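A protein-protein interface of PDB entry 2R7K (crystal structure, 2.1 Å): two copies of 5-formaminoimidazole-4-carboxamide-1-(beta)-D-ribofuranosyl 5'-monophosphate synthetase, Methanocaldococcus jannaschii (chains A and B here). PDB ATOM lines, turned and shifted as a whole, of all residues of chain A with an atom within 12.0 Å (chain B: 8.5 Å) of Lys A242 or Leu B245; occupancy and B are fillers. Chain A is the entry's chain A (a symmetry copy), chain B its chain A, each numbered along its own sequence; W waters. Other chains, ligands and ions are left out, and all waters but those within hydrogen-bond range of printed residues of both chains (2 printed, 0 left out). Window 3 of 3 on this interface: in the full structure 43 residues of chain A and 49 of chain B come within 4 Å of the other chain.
The backbone carbonyl oxygen (O) of Ile B168 lies within hydrogen-bond range of the side-chain amino group (NZ) of Lys B178 (2.5 Å).
The side-chain carboxylate (OE1) of Glu B174 lies within hydrogen-bond range of the backbone NH (N) of Ser B170 (2.8 Å).
The side-chain amino group (NZ) of Lys B178 lies within salt-bridge range of the side-chain carboxylate (OE2) of Glu B174, 3.4 Å away.
The backbone carbonyl oxygen (O) of Leu B236 sits at hydrogen-bond distance from the side-chain amide nitrogen (NE2) of Gln B244 (3.5 Å).
O of Ile B239 sits at hydrogen-bond distance from NE2 of Gln B244.
OE2 of Glu B174 lies close to OE1 of Glu A246 (2.6 Å).
The side-chain carboxylate (OD1) of Asp A243 lies within salt-bridge range of the side-chain amino group (NZ) of Lys B178 (2.7 Å).
OE1 of Gln B244 sits at hydrogen-bond distance from N of Ala A241.
O of Leu B245 is in hydrogen-bond range of NZ of Lys A242, at 3.5 Å.
Among the printed residues, merely in contact across the chains: Pro A240 with Ile B168, Pro A240 with Gln B244, Ala A241 with Ala B241, Lys A242 with Gln B244, Lys A242 with Met B247, Asp A243 with Ile B168, Asp A243 with Glu B174 and Leu A245 with Leu B245.
Of the 15 printed residues of chain A, 6 touch a printed residue of chain B.
Printed residues of chain A that touch a printed residue of chain B: Pro A240, Ala A241, Lys A242, Asp A243, Leu A245 and Glu A246.
Hydrophobic or aromatic side chains of chain A within 4 Å of the printed part of chain B: Pro A240, Ala A241 and Leu A245.
Of the 19 printed residues of chain B, 7 touch a printed residue of chain A.
Printed residues of chain B that touch a printed residue of chain A: Ile B168, Glu B174, Lys B178, Ala B241, Gln B244, Leu B245 and Met B247.
Hydrophobic or aromatic side chains of chain B that line the printed part of chain A: Ile B168, Ala B241 and Leu B245.
Along chain B the printed residues that touch a printed residue of chain A span positions 168 to 247.
Among the printed residues, 12 pairs touch across the chains.
Among the printed residues, Asp or Glu carboxylates within 4 Å of a Lys or Arg side-chain nitrogen of the other chain: Asp A243 with Lys B178 (2.7 Å).
Water W1 lies within hydrogen-bond range of the backbone carbonyl oxygen of Ile A239 (2.9 Å), the side-chain amide nitrogen of Gln B244 (2.9 Å) and the side-chain amide nitrogen of Gln A244 (3.4 Å).
Water W2 lies within hydrogen-bond range of the backbone NH (N) of Lys A242 (3.1 Å), the side-chain amide oxygen (OE1) of Gln B244 (3.2 Å) and the backbone NH (N) of Ala A241 (3.4 Å).
Lys A242 touches just these residues of chain B: Gln B244 (3.4 Å), Leu B245 (3.5 Å) and Met B247 (3.3 Å).
Leu B245 touches just these residues of chain A: Lys A242 and Leu A245.
Of chain B, only Ala B241 (3.9 Å) and Gln B244 (2.9 Å) come within 4 Å of Ala A241.
Of the printed residues of chain A, Ala B241 touches Ala A241 (3.9 Å).
Asp B243 touches none of the printed residues of chain A.
No residue of chain A comes within 4 Å of Glu B246.
Met B247 touches just one residue of chain A: Lys A242 (3.3 Å).
Of the printed residues of chain B, Asp A243 touches Ile B168 (3.7 Å), Glu B174 (3.7 Å) and Lys B178 (2.7 Å).
Of the printed residues of chain A, Lys B178 touches Asp A243.
Of the printed residues of chain B, Glu A246 touches Glu B174 (2.6 Å).
Of the printed residues of chain B, Pro A240 touches Ile B168 (3.7 Å) and Gln B244 (3.6 Å).
Val A237 touches none of the printed residues of chain B.
Asn A248 touches none of the printed residues of chain B.
The nearest residue of chain B that does not touch Lys A242 is Asn B248 (5.1 Å).
The nearest residue of chain A that does not touch Leu B245 is Ala A241 (4.1 Å).
Ala B241 touches its own counterpart, Ala A241.
Ala A241 touches Gln B244, but with the chains exchanged Gln A244 does not touch Ala B241 (6.6 Å).
Lys A242 touches Leu B245, but with the chains exchanged Leu A245 does not touch Lys B242 (8.0 Å).
Leu A245 touches its own counterpart, Leu B245.
Positions printed for both chains: 236, 239, 240, 241, 242, 243, 244, 245, 246, 247, 248 and 249.
Of the 12 pairs that touch across the chains among the printed residues, 2 have their exchanged pair printed and touching as well.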
ATOM      1  N   GLY A 235      15.509   2.141 -19.025  1.00  0.00           N
ATOM      2  CA  GLY A 235      15.993   0.758 -18.946  1.00  0.00           C
ATOM      3  C   GLY A 235      14.857  -0.233 -18.701  1.00  0.00           C
ATOM      4  O   GLY A 235      14.841  -1.319 -19.278  1.00  0.00           O
ATOM      5  N   LEU A 236      13.901   0.154 -17.853  1.00  0.00           N
ATOM      6  CA  LEU A 236      12.762  -0.698 -17.500  1.00  0.00           C
ATOM      7  C   LEU A 236      11.934  -1.087 -18.723  1.00  0.00           C
ATOM      8  O   LEU A 236      11.674  -2.266 -18.953  1.00  0.00           O
ATOM      9  CB  LEU A 236      11.879  -0.001 -16.451  1.00  0.00           C
ATOM     10  CG  LEU A 236      10.601  -0.694 -15.949  1.00  0.00           C
ATOM     11  CD1 LEU A 236      10.847  -2.165 -15.695  1.00  0.00           C
ATOM     12  CD2 LEU A 236      10.088  -0.008 -14.673  1.00  0.00           C
ATOM     13  N   VAL A 237      11.538  -0.091 -19.508  1.00  0.00           N
ATOM     14  CA  VAL A 237      10.698  -0.308 -20.680  1.00  0.00           C
ATOM     15  C   VAL A 237      11.449  -0.954 -21.836  1.00  0.00           C
ATOM     16  O   VAL A 237      10.867  -1.244 -22.882  1.00  0.00           O
ATOM     17  CB  VAL A 237      10.037   0.995 -21.144  1.00  0.00           C
ATOM     18  CG1 VAL A 237       9.191   1.571 -20.011  1.00  0.00           C
ATOM     19  CG2 VAL A 237      11.095   2.008 -21.585  1.00  0.00           C
ATOM     20  N   ARG A 238      12.734  -1.214 -21.637  1.00  0.00           N
ATOM     21  CA  ARG A 238      13.516  -1.914 -22.647  1.00  0.00           C
ATOM     22  C   ARG A 238      13.558  -3.409 -22.342  1.00  0.00           C
ATOM     23  O   ARG A 238      14.190  -4.184 -23.062  1.00  0.00           O
ATOM     24  CB  ARG A 238      14.939  -1.354 -22.730  1.00  0.00           C
ATOM     25  CG  ARG A 238      15.529  -1.429 -24.134  1.00  0.00           C
ATOM     26  CD  ARG A 238      16.980  -1.810 -24.106  1.00  0.00           C
ATOM     27  NE  ARG A 238      17.544  -1.900 -25.450  1.00  0.00           N
ATOM     28  CZ  ARG A 238      18.614  -2.621 -25.760  1.00  0.00           C
ATOM     29  NH1 ARG A 238      19.227  -3.333 -24.825  1.00  0.00           N
ATOM     30  NH2 ARG A 238      19.070  -2.635 -27.005  1.00  0.00           N
ATOM     31  N   ILE A 239      12.891  -3.798 -21.259  1.00  0.00           N
ATOM     32  CA  ILE A 239      12.722  -5.211 -20.887  1.00  0.00           C
ATOM     33  C   ILE A 239      11.409  -5.694 -21.501  1.00  0.00           C
ATOM     34  O   ILE A 239      10.395  -5.007 -21.397  1.00  0.00           O
ATOM     35  CB  ILE A 239      12.653  -5.357 -19.350  1.00  0.00           C
ATOM     36  CG1 ILE A 239      13.961  -4.892 -18.715  1.00  0.00           C
ATOM     37  CG2 ILE A 239      12.353  -6.802 -18.937  1.00  0.00           C
ATOM     38  CD1 ILE A 239      13.879  -4.715 -17.211  1.00  0.00           C
ATOM     39  N   PRO A 240      11.423  -6.850 -22.189  1.00  0.00           N
ATOM     40  CA  PRO A 240      10.174  -7.343 -22.798  1.00  0.00           C
ATOM     41  C   PRO A 240       9.070  -7.499 -21.750  1.00  0.00           C
ATOM     42  O   PRO A 240       9.360  -7.815 -20.602  1.00  0.00           O
ATOM     43  CB  PRO A 240      10.573  -8.701 -23.372  1.00  0.00           C
ATOM     44  CG  PRO A 240      12.049  -8.588 -23.597  1.00  0.00           C
ATOM     45  CD  PRO A 240      12.559  -7.740 -22.470  1.00  0.00           C
ATOM     46  N   ALA A 241       7.828  -7.240 -22.149  1.00  0.00           N
ATOM     47  CA  ALA A 241       6.686  -7.226 -21.228  1.00  0.00           C
ATOM     48  C   ALA A 241       6.594  -8.490 -20.368  1.00  0.00           C
ATOM     49  O   ALA A 241       6.375  -8.408 -19.156  1.00  0.00           O
ATOM     50  CB  ALA A 241       5.394  -7.009 -21.995  1.00  0.00           C
ATOM     51  N   LYS A 242       6.781  -9.648 -20.995  1.00  0.00           N
ATOM     52  CA  LYS A 242       6.701 -10.930 -20.287  1.00  0.00           C
ATOM     53  C   LYS A 242       7.680 -10.994 -19.124  1.00  0.00           C
ATOM     54  O   LYS A 242       7.346 -11.478 -18.048  1.00  0.00           O
ATOM     55  CB  LYS A 242       6.934 -12.093 -21.250  1.00  0.00           C
ATOM     56  CG  LYS A 242       5.725 -12.404 -22.127  1.00  0.00           C
ATOM     57  CD  LYS A 242       6.128 -13.179 -23.369  1.00  0.00           C
ATOM     58  CE  LYS A 242       4.955 -13.359 -24.323  1.00  0.00           C
ATOM     59  NZ  LYS A 242       4.063 -14.474 -23.912  1.00  0.00           N
ATOM     60  N   ASP A 243       8.887 -10.486 -19.335  1.00  0.00           N
ATOM     61  CA  ASP A 243       9.861 -10.396 -18.251  1.00  0.00           C
ATOM     62  C   ASP A 243       9.557  -9.287 -17.241  1.00  0.00           C
ATOM     63  O   ASP A 243       9.819  -9.442 -16.052  1.00  0.00           O
ATOM     64  CB  ASP A 243      11.262 -10.244 -18.833  1.00  0.00           C
ATOM     65  CG  ASP A 243      11.610 -11.374 -19.767  1.00  0.00           C
ATOM     66  OD1 ASP A 243      11.640 -12.528 -19.294  1.00  0.00           O
ATOM     67  OD2 ASP A 243      11.832 -11.122 -20.970  1.00  0.00           O
ATOM     68  N   GLN A 244       9.004  -8.166 -17.695  1.00  0.00           N
ATOM     69  CA  GLN A 244       8.656  -7.101 -16.758  1.00  0.00           C
ATOM     70  C   GLN A 244       7.625  -7.592 -15.741  1.00  0.00           C
ATOM     71  O   GLN A 244       7.670  -7.221 -14.570  1.00  0.00           O
ATOM     72  CB  GLN A 244       8.082  -5.894 -17.485  1.00  0.00           C
ATOM     73  CG  GLN A 244       9.101  -4.962 -18.109  1.00  0.00           C
ATOM     74  CD  GLN A 244       8.426  -3.736 -18.664  1.00  0.00           C
ATOM     75  OE1 GLN A 244       7.752  -3.007 -17.932  1.00  0.00           O
ATOM     76  NE2 GLN A 244       8.572  -3.513 -19.967  1.00  0.00           N
ATOM     77  N   LEU A 245       6.684  -8.409 -16.208  1.00  0.00           N
ATOM     78  CA  LEU A 245       5.635  -8.956 -15.347  1.00  0.00           C
ATOM     79  C   LEU A 245       6.182  -9.911 -14.295  1.00  0.00           C
ATOM     80  O   LEU A 245       5.578 -10.085 -13.241  1.00  0.00           O
ATOM     81  CB  LEU A 245       4.551  -9.654 -16.176  1.00  0.00           C
ATOM     82  CG  LEU A 245       3.843  -8.736 -17.171  1.00  0.00           C
ATOM     83  CD1 LEU A 245       2.636  -9.433 -17.776  1.00  0.00           C
ATOM     84  CD2 LEU A 245       3.443  -7.422 -16.515  1.00  0.00           C
ATOM     85  N   GLU A 246       7.325 -10.523 -14.578  1.00  0.00           N
ATOM     86  CA  GLU A 246       7.958 -11.417 -13.620  1.00  0.00           C
ATOM     87  C   GLU A 246       8.830 -10.689 -12.610  1.00  0.00           C
ATOM     88  O   GLU A 246       9.425 -11.320 -11.740  1.00  0.00           O
ATOM     89  CB  GLU A 246       8.802 -12.458 -14.340  1.00  0.00           C
ATOM     90  CG  GLU A 246       7.994 -13.576 -14.944  1.00  0.00           C
ATOM     91  CD  GLU A 246       8.851 -14.506 -15.759  1.00  0.00           C
ATOM     92  OE1 GLU A 246       9.479 -14.032 -16.730  1.00  0.00           O
ATOM     93  OE2 GLU A 246       8.899 -15.710 -15.426  1.00  0.00           O
ATOM     94  N   MET A 247       8.919  -9.368 -12.726  1.00  0.00           N
ATOM     95  CA  MET A 247       9.809  -8.603 -11.858  1.00  0.00           C
ATOM     96  C   MET A 247       9.025  -7.771 -10.851  1.00  0.00           C
ATOM     97  O   MET A 247       7.882  -7.375 -11.101  1.00  0.00           O
ATOM     98  CB  MET A 247      10.712  -7.675 -12.682  1.00  0.00           C
ATOM     99  CG  MET A 247      11.493  -8.358 -13.795  1.00  0.00           C
ATOM    100  SD  MET A 247      12.270  -7.161 -14.908  1.00  0.00           S
ATOM    101  CE  MET A 247      13.497  -6.433 -13.820  1.00  0.00           C
ATOM    102  N   ASN A 248       9.648  -7.511  -9.710  1.00  0.00           N
ATOM    103  CA  ASN A 248       9.087  -6.584  -8.744  1.00  0.00           C
ATOM    104  C   ASN A 248       9.912  -5.313  -8.804  1.00  0.00           C
ATOM    105  O   ASN A 248      10.843  -5.127  -8.024  1.00  0.00           O
ATOM    106  CB  ASN A 248       9.102  -7.178  -7.332  1.00  0.00           C
ATOM    107  CG  ASN A 248       8.361  -8.506  -7.247  1.00  0.00           C
ATOM    108  OD1 ASN A 248       7.236  -8.638  -7.737  1.00  0.00           O
ATOM    109  ND2 ASN A 248       8.993  -9.499  -6.622  1.00  0.00           N
ATOM    110  N   ILE A 249       9.578  -4.446  -9.752  1.00  0.00           N
ATOM    111  CA  ILE A 249      10.400  -3.273  -9.996  1.00  0.00           C
ATOM    112  C   ILE A 249       9.547  -2.025 -10.174  1.00  0.00           C
ATOM    113  O   ILE A 249       8.574  -2.023 -10.931  1.00  0.00           O
ATOM    114  CB  ILE A 249      11.318  -3.495 -11.227  1.00  0.00           C
ATOM    115  CG1 ILE A 249      12.299  -2.329 -11.400  1.00  0.00           C
ATOM    116  CG2 ILE A 249      10.483  -3.742 -12.485  1.00  0.00           C
ATOM    117  CD1 ILE A 249      13.324  -2.553 -12.493  1.00  0.00           C
ATOM    118  N   ILE B 168      16.456 -13.540 -20.904  1.00  0.00           N
ATOM    119  CA  ILE B 168      16.331 -12.965 -19.573  1.00  0.00           C
ATOM    120  C   ILE B 168      15.603 -13.953 -18.659  1.00  0.00           C
ATOM    121  O   ILE B 168      14.649 -14.609 -19.082  1.00  0.00           O
ATOM    122  CB  ILE B 168      15.524 -11.649 -19.627  1.00  0.00           C
ATOM    123  CG1 ILE B 168      16.235 -10.630 -20.530  1.00  0.00           C
ATOM    124  CG2 ILE B 168      15.291 -11.092 -18.225  1.00  0.00           C
ATOM    125  CD1 ILE B 168      15.437  -9.361 -20.785  1.00  0.00           C
ATOM    126  N   SER B 170      14.295 -14.677 -14.353  1.00  0.00           N
ATOM    127  CA  SER B 170      14.157 -14.218 -12.969  1.00  0.00           C
ATOM    128  C   SER B 170      14.152 -15.359 -11.939  1.00  0.00           C
ATOM    129  O   SER B 170      14.012 -15.112 -10.736  1.00  0.00           O
ATOM    130  CB  SER B 170      12.915 -13.337 -12.803  1.00  0.00           C
ATOM    131  OG  SER B 170      13.094 -12.071 -13.423  1.00  0.00           O
ATOM    132  N   GLU B 174      12.835 -20.623 -14.610  1.00  0.00           N
ATOM    133  CA  GLU B 174      12.704 -19.899 -15.866  1.00  0.00           C
ATOM    134  C   GLU B 174      13.932 -20.093 -16.755  1.00  0.00           C
ATOM    135  O   GLU B 174      13.811 -20.266 -17.967  1.00  0.00           O
ATOM    136  CB  GLU B 174      12.449 -18.413 -15.627  1.00  0.00           C
ATOM    137  CG  GLU B 174      12.364 -17.632 -16.921  1.00  0.00           C
ATOM    138  CD  GLU B 174      11.750 -16.267 -16.750  1.00  0.00           C
ATOM    139  OE1 GLU B 174      11.985 -15.625 -15.701  1.00  0.00           O
ATOM    140  OE2 GLU B 174      11.036 -15.838 -17.678  1.00  0.00           O
ATOM    141  N   LYS B 177      13.417 -23.366 -18.559  1.00  0.00           N
ATOM    142  CA  LYS B 177      12.302 -23.227 -19.486  1.00  0.00           C
ATOM    143  C   LYS B 177      12.803 -22.585 -20.780  1.00  0.00           C
ATOM    144  O   LYS B 177      12.569 -23.100 -21.876  1.00  0.00           O
ATOM    145  CB  LYS B 177      11.189 -22.385 -18.853  1.00  0.00           C
ATOM    146  CG  LYS B 177       9.832 -22.487 -19.544  1.00  0.00           C
ATOM    147  CD  LYS B 177       9.727 -21.560 -20.752  1.00  0.00           C
ATOM    148  CE  LYS B 177       8.330 -21.595 -21.357  1.00  0.00           C
ATOM    149  NZ  LYS B 177       8.225 -20.726 -22.564  1.00  0.00           N
ATOM    150  N   LYS B 178      13.520 -21.472 -20.638  1.00  0.00           N
ATOM    151  CA  LYS B 178      13.997 -20.702 -21.790  1.00  0.00           C
ATOM    152  C   LYS B 178      15.162 -21.351 -22.538  1.00  0.00           C
ATOM    153  O   LYS B 178      15.195 -21.351 -23.772  1.00  0.00           O
ATOM    154  CB  LYS B 178      14.335 -19.269 -21.372  1.00  0.00           C
ATOM    155  CG  LYS B 178      13.102 -18.385 -21.302  1.00  0.00           C
ATOM    156  CD  LYS B 178      13.371 -17.077 -20.601  1.00  0.00           C
ATOM    157  CE  LYS B 178      12.211 -16.132 -20.829  1.00  0.00           C
ATOM    158  NZ  LYS B 178      12.568 -14.740 -20.464  1.00  0.00           N
ATOM    159  N   LEU B 236      11.090  -5.060 -30.488  1.00  0.00           N
ATOM    160  CA  LEU B 236      10.206  -5.825 -29.603  1.00  0.00           C
ATOM    161  C   LEU B 236       9.525  -4.937 -28.564  1.00  0.00           C
ATOM    162  O   LEU B 236       8.304  -4.960 -28.426  1.00  0.00           O
ATOM    163  CB  LEU B 236      10.988  -6.956 -28.915  1.00  0.00           C
ATOM    164  CG  LEU B 236      10.273  -7.877 -27.912  1.00  0.00           C
ATOM    165  CD1 LEU B 236       8.903  -8.268 -28.418  1.00  0.00           C
ATOM    166  CD2 LEU B 236      11.121  -9.128 -27.637  1.00  0.00           C
ATOM    167  N   ILE B 239       6.513  -2.664 -29.242  1.00  0.00           N
ATOM    168  CA  ILE B 239       5.179  -3.271 -29.372  1.00  0.00           C
ATOM    169  C   ILE B 239       4.467  -3.107 -28.031  1.00  0.00           C
ATOM    170  O   ILE B 239       5.058  -3.374 -26.987  1.00  0.00           O
ATOM    171  CB  ILE B 239       5.304  -4.775 -29.704  1.00  0.00           C
ATOM    172  CG1 ILE B 239       6.002  -4.964 -31.049  1.00  0.00           C
ATOM    173  CG2 ILE B 239       3.933  -5.460 -29.724  1.00  0.00           C
ATOM    174  CD1 ILE B 239       6.436  -6.392 -31.315  1.00  0.00           C
ATOM    175  N   PRO B 240       3.214  -2.617 -28.039  1.00  0.00           N
ATOM    176  CA  PRO B 240       2.500  -2.442 -26.762  1.00  0.00           C
ATOM    177  C   PRO B 240       2.424  -3.757 -25.983  1.00  0.00           C
ATOM    178  O   PRO B 240       2.348  -4.820 -26.588  1.00  0.00           O
ATOM    179  CB  PRO B 240       1.106  -1.988 -27.196  1.00  0.00           C
ATOM    180  CG  PRO B 240       1.323  -1.365 -28.540  1.00  0.00           C
ATOM    181  CD  PRO B 240       2.405  -2.178 -29.186  1.00  0.00           C
ATOM    182  N   ALA B 241       2.483  -3.669 -24.657  1.00  0.00           N
ATOM    183  CA  ALA B 241       2.549  -4.849 -23.787  1.00  0.00           C
ATOM    184  C   ALA B 241       1.456  -5.878 -24.089  1.00  0.00           C
ATOM    185  O   ALA B 241       1.731  -7.078 -24.165  1.00  0.00           O
ATOM    186  CB  ALA B 241       2.496  -4.429 -22.328  1.00  0.00           C
ATOM    187  N   LYS B 242       0.229  -5.400 -24.279  1.00  0.00           N
ATOM    188  CA  LYS B 242      -0.907  -6.285 -24.558  1.00  0.00           C
ATOM    189  C   LYS B 242      -0.666  -7.142 -25.791  1.00  0.00           C
ATOM    190  O   LYS B 242      -0.981  -8.327 -25.805  1.00  0.00           O
ATOM    191  CB  LYS B 242      -2.195  -5.476 -24.709  1.00  0.00           C
ATOM    192  CG  LYS B 242      -2.776  -5.007 -23.379  1.00  0.00           C
ATOM    193  CD  LYS B 242      -3.717  -3.832 -23.570  1.00  0.00           C
ATOM    194  CE  LYS B 242      -4.179  -3.261 -22.236  1.00  0.00           C
ATOM    195  NZ  LYS B 242      -5.286  -4.053 -21.639  1.00  0.00           N
ATOM    196  N   ASP B 243      -0.087  -6.545 -26.826  1.00  0.00           N
ATOM    197  CA  ASP B 243       0.292  -7.305 -28.013  1.00  0.00           C
ATOM    198  C   ASP B 243       1.528  -8.186 -27.812  1.00  0.00           C
ATOM    199  O   ASP B 243       1.613  -9.272 -28.378  1.00  0.00           O
ATOM    200  CB  ASP B 243       0.474  -6.356 -29.191  1.00  0.00           C
ATOM    201  CG  ASP B 243      -0.764  -5.539 -29.456  1.00  0.00           C
ATOM    202  OD1 ASP B 243      -1.806  -6.151 -29.765  1.00  0.00           O
ATOM    203  OD2 ASP B 243      -0.710  -4.297 -29.337  1.00  0.00           O
ATOM    204  N   GLN B 244       2.489  -7.735 -27.012  1.00  0.00           N
ATOM    205  CA  GLN B 244       3.664  -8.565 -26.758  1.00  0.00           C
ATOM    206  C   GLN B 244       3.263  -9.879 -26.088  1.00  0.00           C
ATOM    207  O   GLN B 244       3.839 -10.928 -26.367  1.00  0.00           O
ATOM    208  CB  GLN B 244       4.660  -7.847 -25.857  1.00  0.00           C
ATOM    209  CG  GLN B 244       5.561  -6.845 -26.548  1.00  0.00           C
ATOM    210  CD  GLN B 244       6.595  -6.315 -25.591  1.00  0.00           C
ATOM    211  OE1 GLN B 244       7.373  -7.085 -25.021  1.00  0.00           O
ATOM    212  NE2 GLN B 244       6.595  -5.002 -25.378  1.00  0.00           N
ATOM    213  N   LEU B 245       2.287  -9.805 -25.187  1.00  0.00           N
ATOM    214  CA  LEU B 245       1.801 -10.985 -24.470  1.00  0.00           C
ATOM    215  C   LEU B 245       1.109 -11.982 -25.389  1.00  0.00           C
ATOM    216  O   LEU B 245       1.067 -13.172 -25.093  1.00  0.00           O
ATOM    217  CB  LEU B 245       0.863 -10.586 -23.327  1.00  0.00           C
ATOM    218  CG  LEU B 245       1.513  -9.691 -22.273  1.00  0.00           C
ATOM    219  CD1 LEU B 245       0.604  -9.539 -21.065  1.00  0.00           C
ATOM    220  CD2 LEU B 245       2.876 -10.229 -21.864  1.00  0.00           C
ATOM    221  N   GLU B 246       0.572 -11.498 -26.502  1.00  0.00           N
ATOM    222  CA  GLU B 246      -0.070 -12.374 -27.472  1.00  0.00           C
ATOM    223  C   GLU B 246       0.909 -12.997 -28.454  1.00  0.00           C
ATOM    224  O   GLU B 246       0.506 -13.761 -29.327  1.00  0.00           O
ATOM    225  CB  GLU B 246      -1.134 -11.616 -28.251  1.00  0.00           C
ATOM    226  CG  GLU B 246      -2.417 -11.419 -27.487  1.00  0.00           C
ATOM    227  CD  GLU B 246      -3.388 -10.552 -28.240  1.00  0.00           C
ATOM    228  OE1 GLU B 246      -3.035  -9.389 -28.536  1.00  0.00           O
ATOM    229  OE2 GLU B 246      -4.502 -11.033 -28.539  1.00  0.00           O
ATOM    230  N   MET B 247       2.191 -12.669 -28.323  1.00  0.00           N
ATOM    231  CA  MET B 247       3.184 -13.147 -29.281  1.00  0.00           C
ATOM    232  C   MET B 247       4.100 -14.192 -28.658  1.00  0.00           C
ATOM    233  O   MET B 247       4.330 -14.200 -27.445  1.00  0.00           O
ATOM    234  CB  MET B 247       4.034 -11.985 -29.812  1.00  0.00           C
ATOM    235  CG  MET B 247       3.244 -10.817 -30.384  1.00  0.00           C
ATOM    236  SD  MET B 247       4.294  -9.375 -30.686  1.00  0.00           S
ATOM    237  CE  MET B 247       5.323  -9.978 -32.027  1.00  0.00           C
ATOM    238  N   ASN B 248       4.620 -15.075 -29.499  1.00  0.00           N
ATOM    239  CA  ASN B 248       5.644 -16.008 -29.067  1.00  0.00           C
ATOM    240  C   ASN B 248       6.959 -15.546 -29.663  1.00  0.00           C
ATOM    241  O   ASN B 248       7.373 -16.014 -30.722  1.00  0.00           O
ATOM    242  CB  ASN B 248       5.316 -17.437 -29.514  1.00  0.00           C
ATOM    243  CG  ASN B 248       3.958 -17.910 -29.012  1.00  0.00           C
ATOM    244  OD1 ASN B 248       3.630 -17.762 -27.832  1.00  0.00           O
ATOM    245  ND2 ASN B 248       3.161 -18.483 -29.913  1.00  0.00           N
ATOM    246  N   ILE B 249       7.606 -14.604 -28.988  1.00  0.00           N
ATOM    247  CA  ILE B 249       8.792 -13.980 -29.549  1.00  0.00           C
ATOM    248  C   ILE B 249       9.897 -13.854 -28.511  1.00  0.00           C
ATOM    249  O   ILE B 249       9.668 -13.392 -27.391  1.00  0.00           O
ATOM    250  CB  ILE B 249       8.445 -12.596 -30.159  1.00  0.00           C
ATOM    251  CG1 ILE B 249       9.654 -11.999 -30.890  1.00  0.00           C
ATOM    252  CG2 ILE B 249       7.896 -11.655 -29.083  1.00  0.00           C
ATOM    253  CD1 ILE B 249       9.341 -10.717 -31.636  1.00  0.00           C
ATOM    254  N   ASN B 250      11.097 -14.281 -28.878  1.00  0.00           N
ATOM    255  CA  ASN B 250      12.248 -14.119 -28.001  1.00  0.00           C
ATOM    256  C   ASN B 250      13.071 -12.900 -28.402  1.00  0.00           C
ATOM    257  O   ASN B 250      13.244 -12.633 -29.594  1.00  0.00           O
ATOM    258  CB  ASN B 250      13.124 -15.369 -28.032  1.00  0.00           C
ATOM    259  CG  ASN B 250      12.365 -16.620 -27.637  1.00  0.00           C
ATOM    260  OD1 ASN B 250      12.430 -17.638 -28.325  1.00  0.00           O
ATOM    261  ND2 ASN B 250      11.631 -16.545 -26.531  1.00  0.00           N
ATOM    262  N   PRO B 251      13.573 -12.154 -27.407  1.00  0.00           N
ATOM    263  CA  PRO B 251      14.441 -11.008 -27.664  1.00  0.00           C
ATOM    264  C   PRO B 251      15.806 -11.424 -28.193  1.00  0.00           C
ATOM    265  O   PRO B 251      16.423 -12.361 -27.677  1.00  0.00           O
ATOM    266  CB  PRO B 251      14.599 -10.366 -26.282  1.00  0.00           C
ATOM    267  CG  PRO B 251      14.389 -11.485 -25.322  1.00  0.00           C
ATOM    268  CD  PRO B 251      13.332 -12.349 -25.966  1.00  0.00           C
HETATM  269  O   HOH W   1       8.527  -4.032 -23.375  1.00  0.00           O
HETATM  270  O   HOH W   2       7.341 -10.078 -24.018  1.00  0.00           O
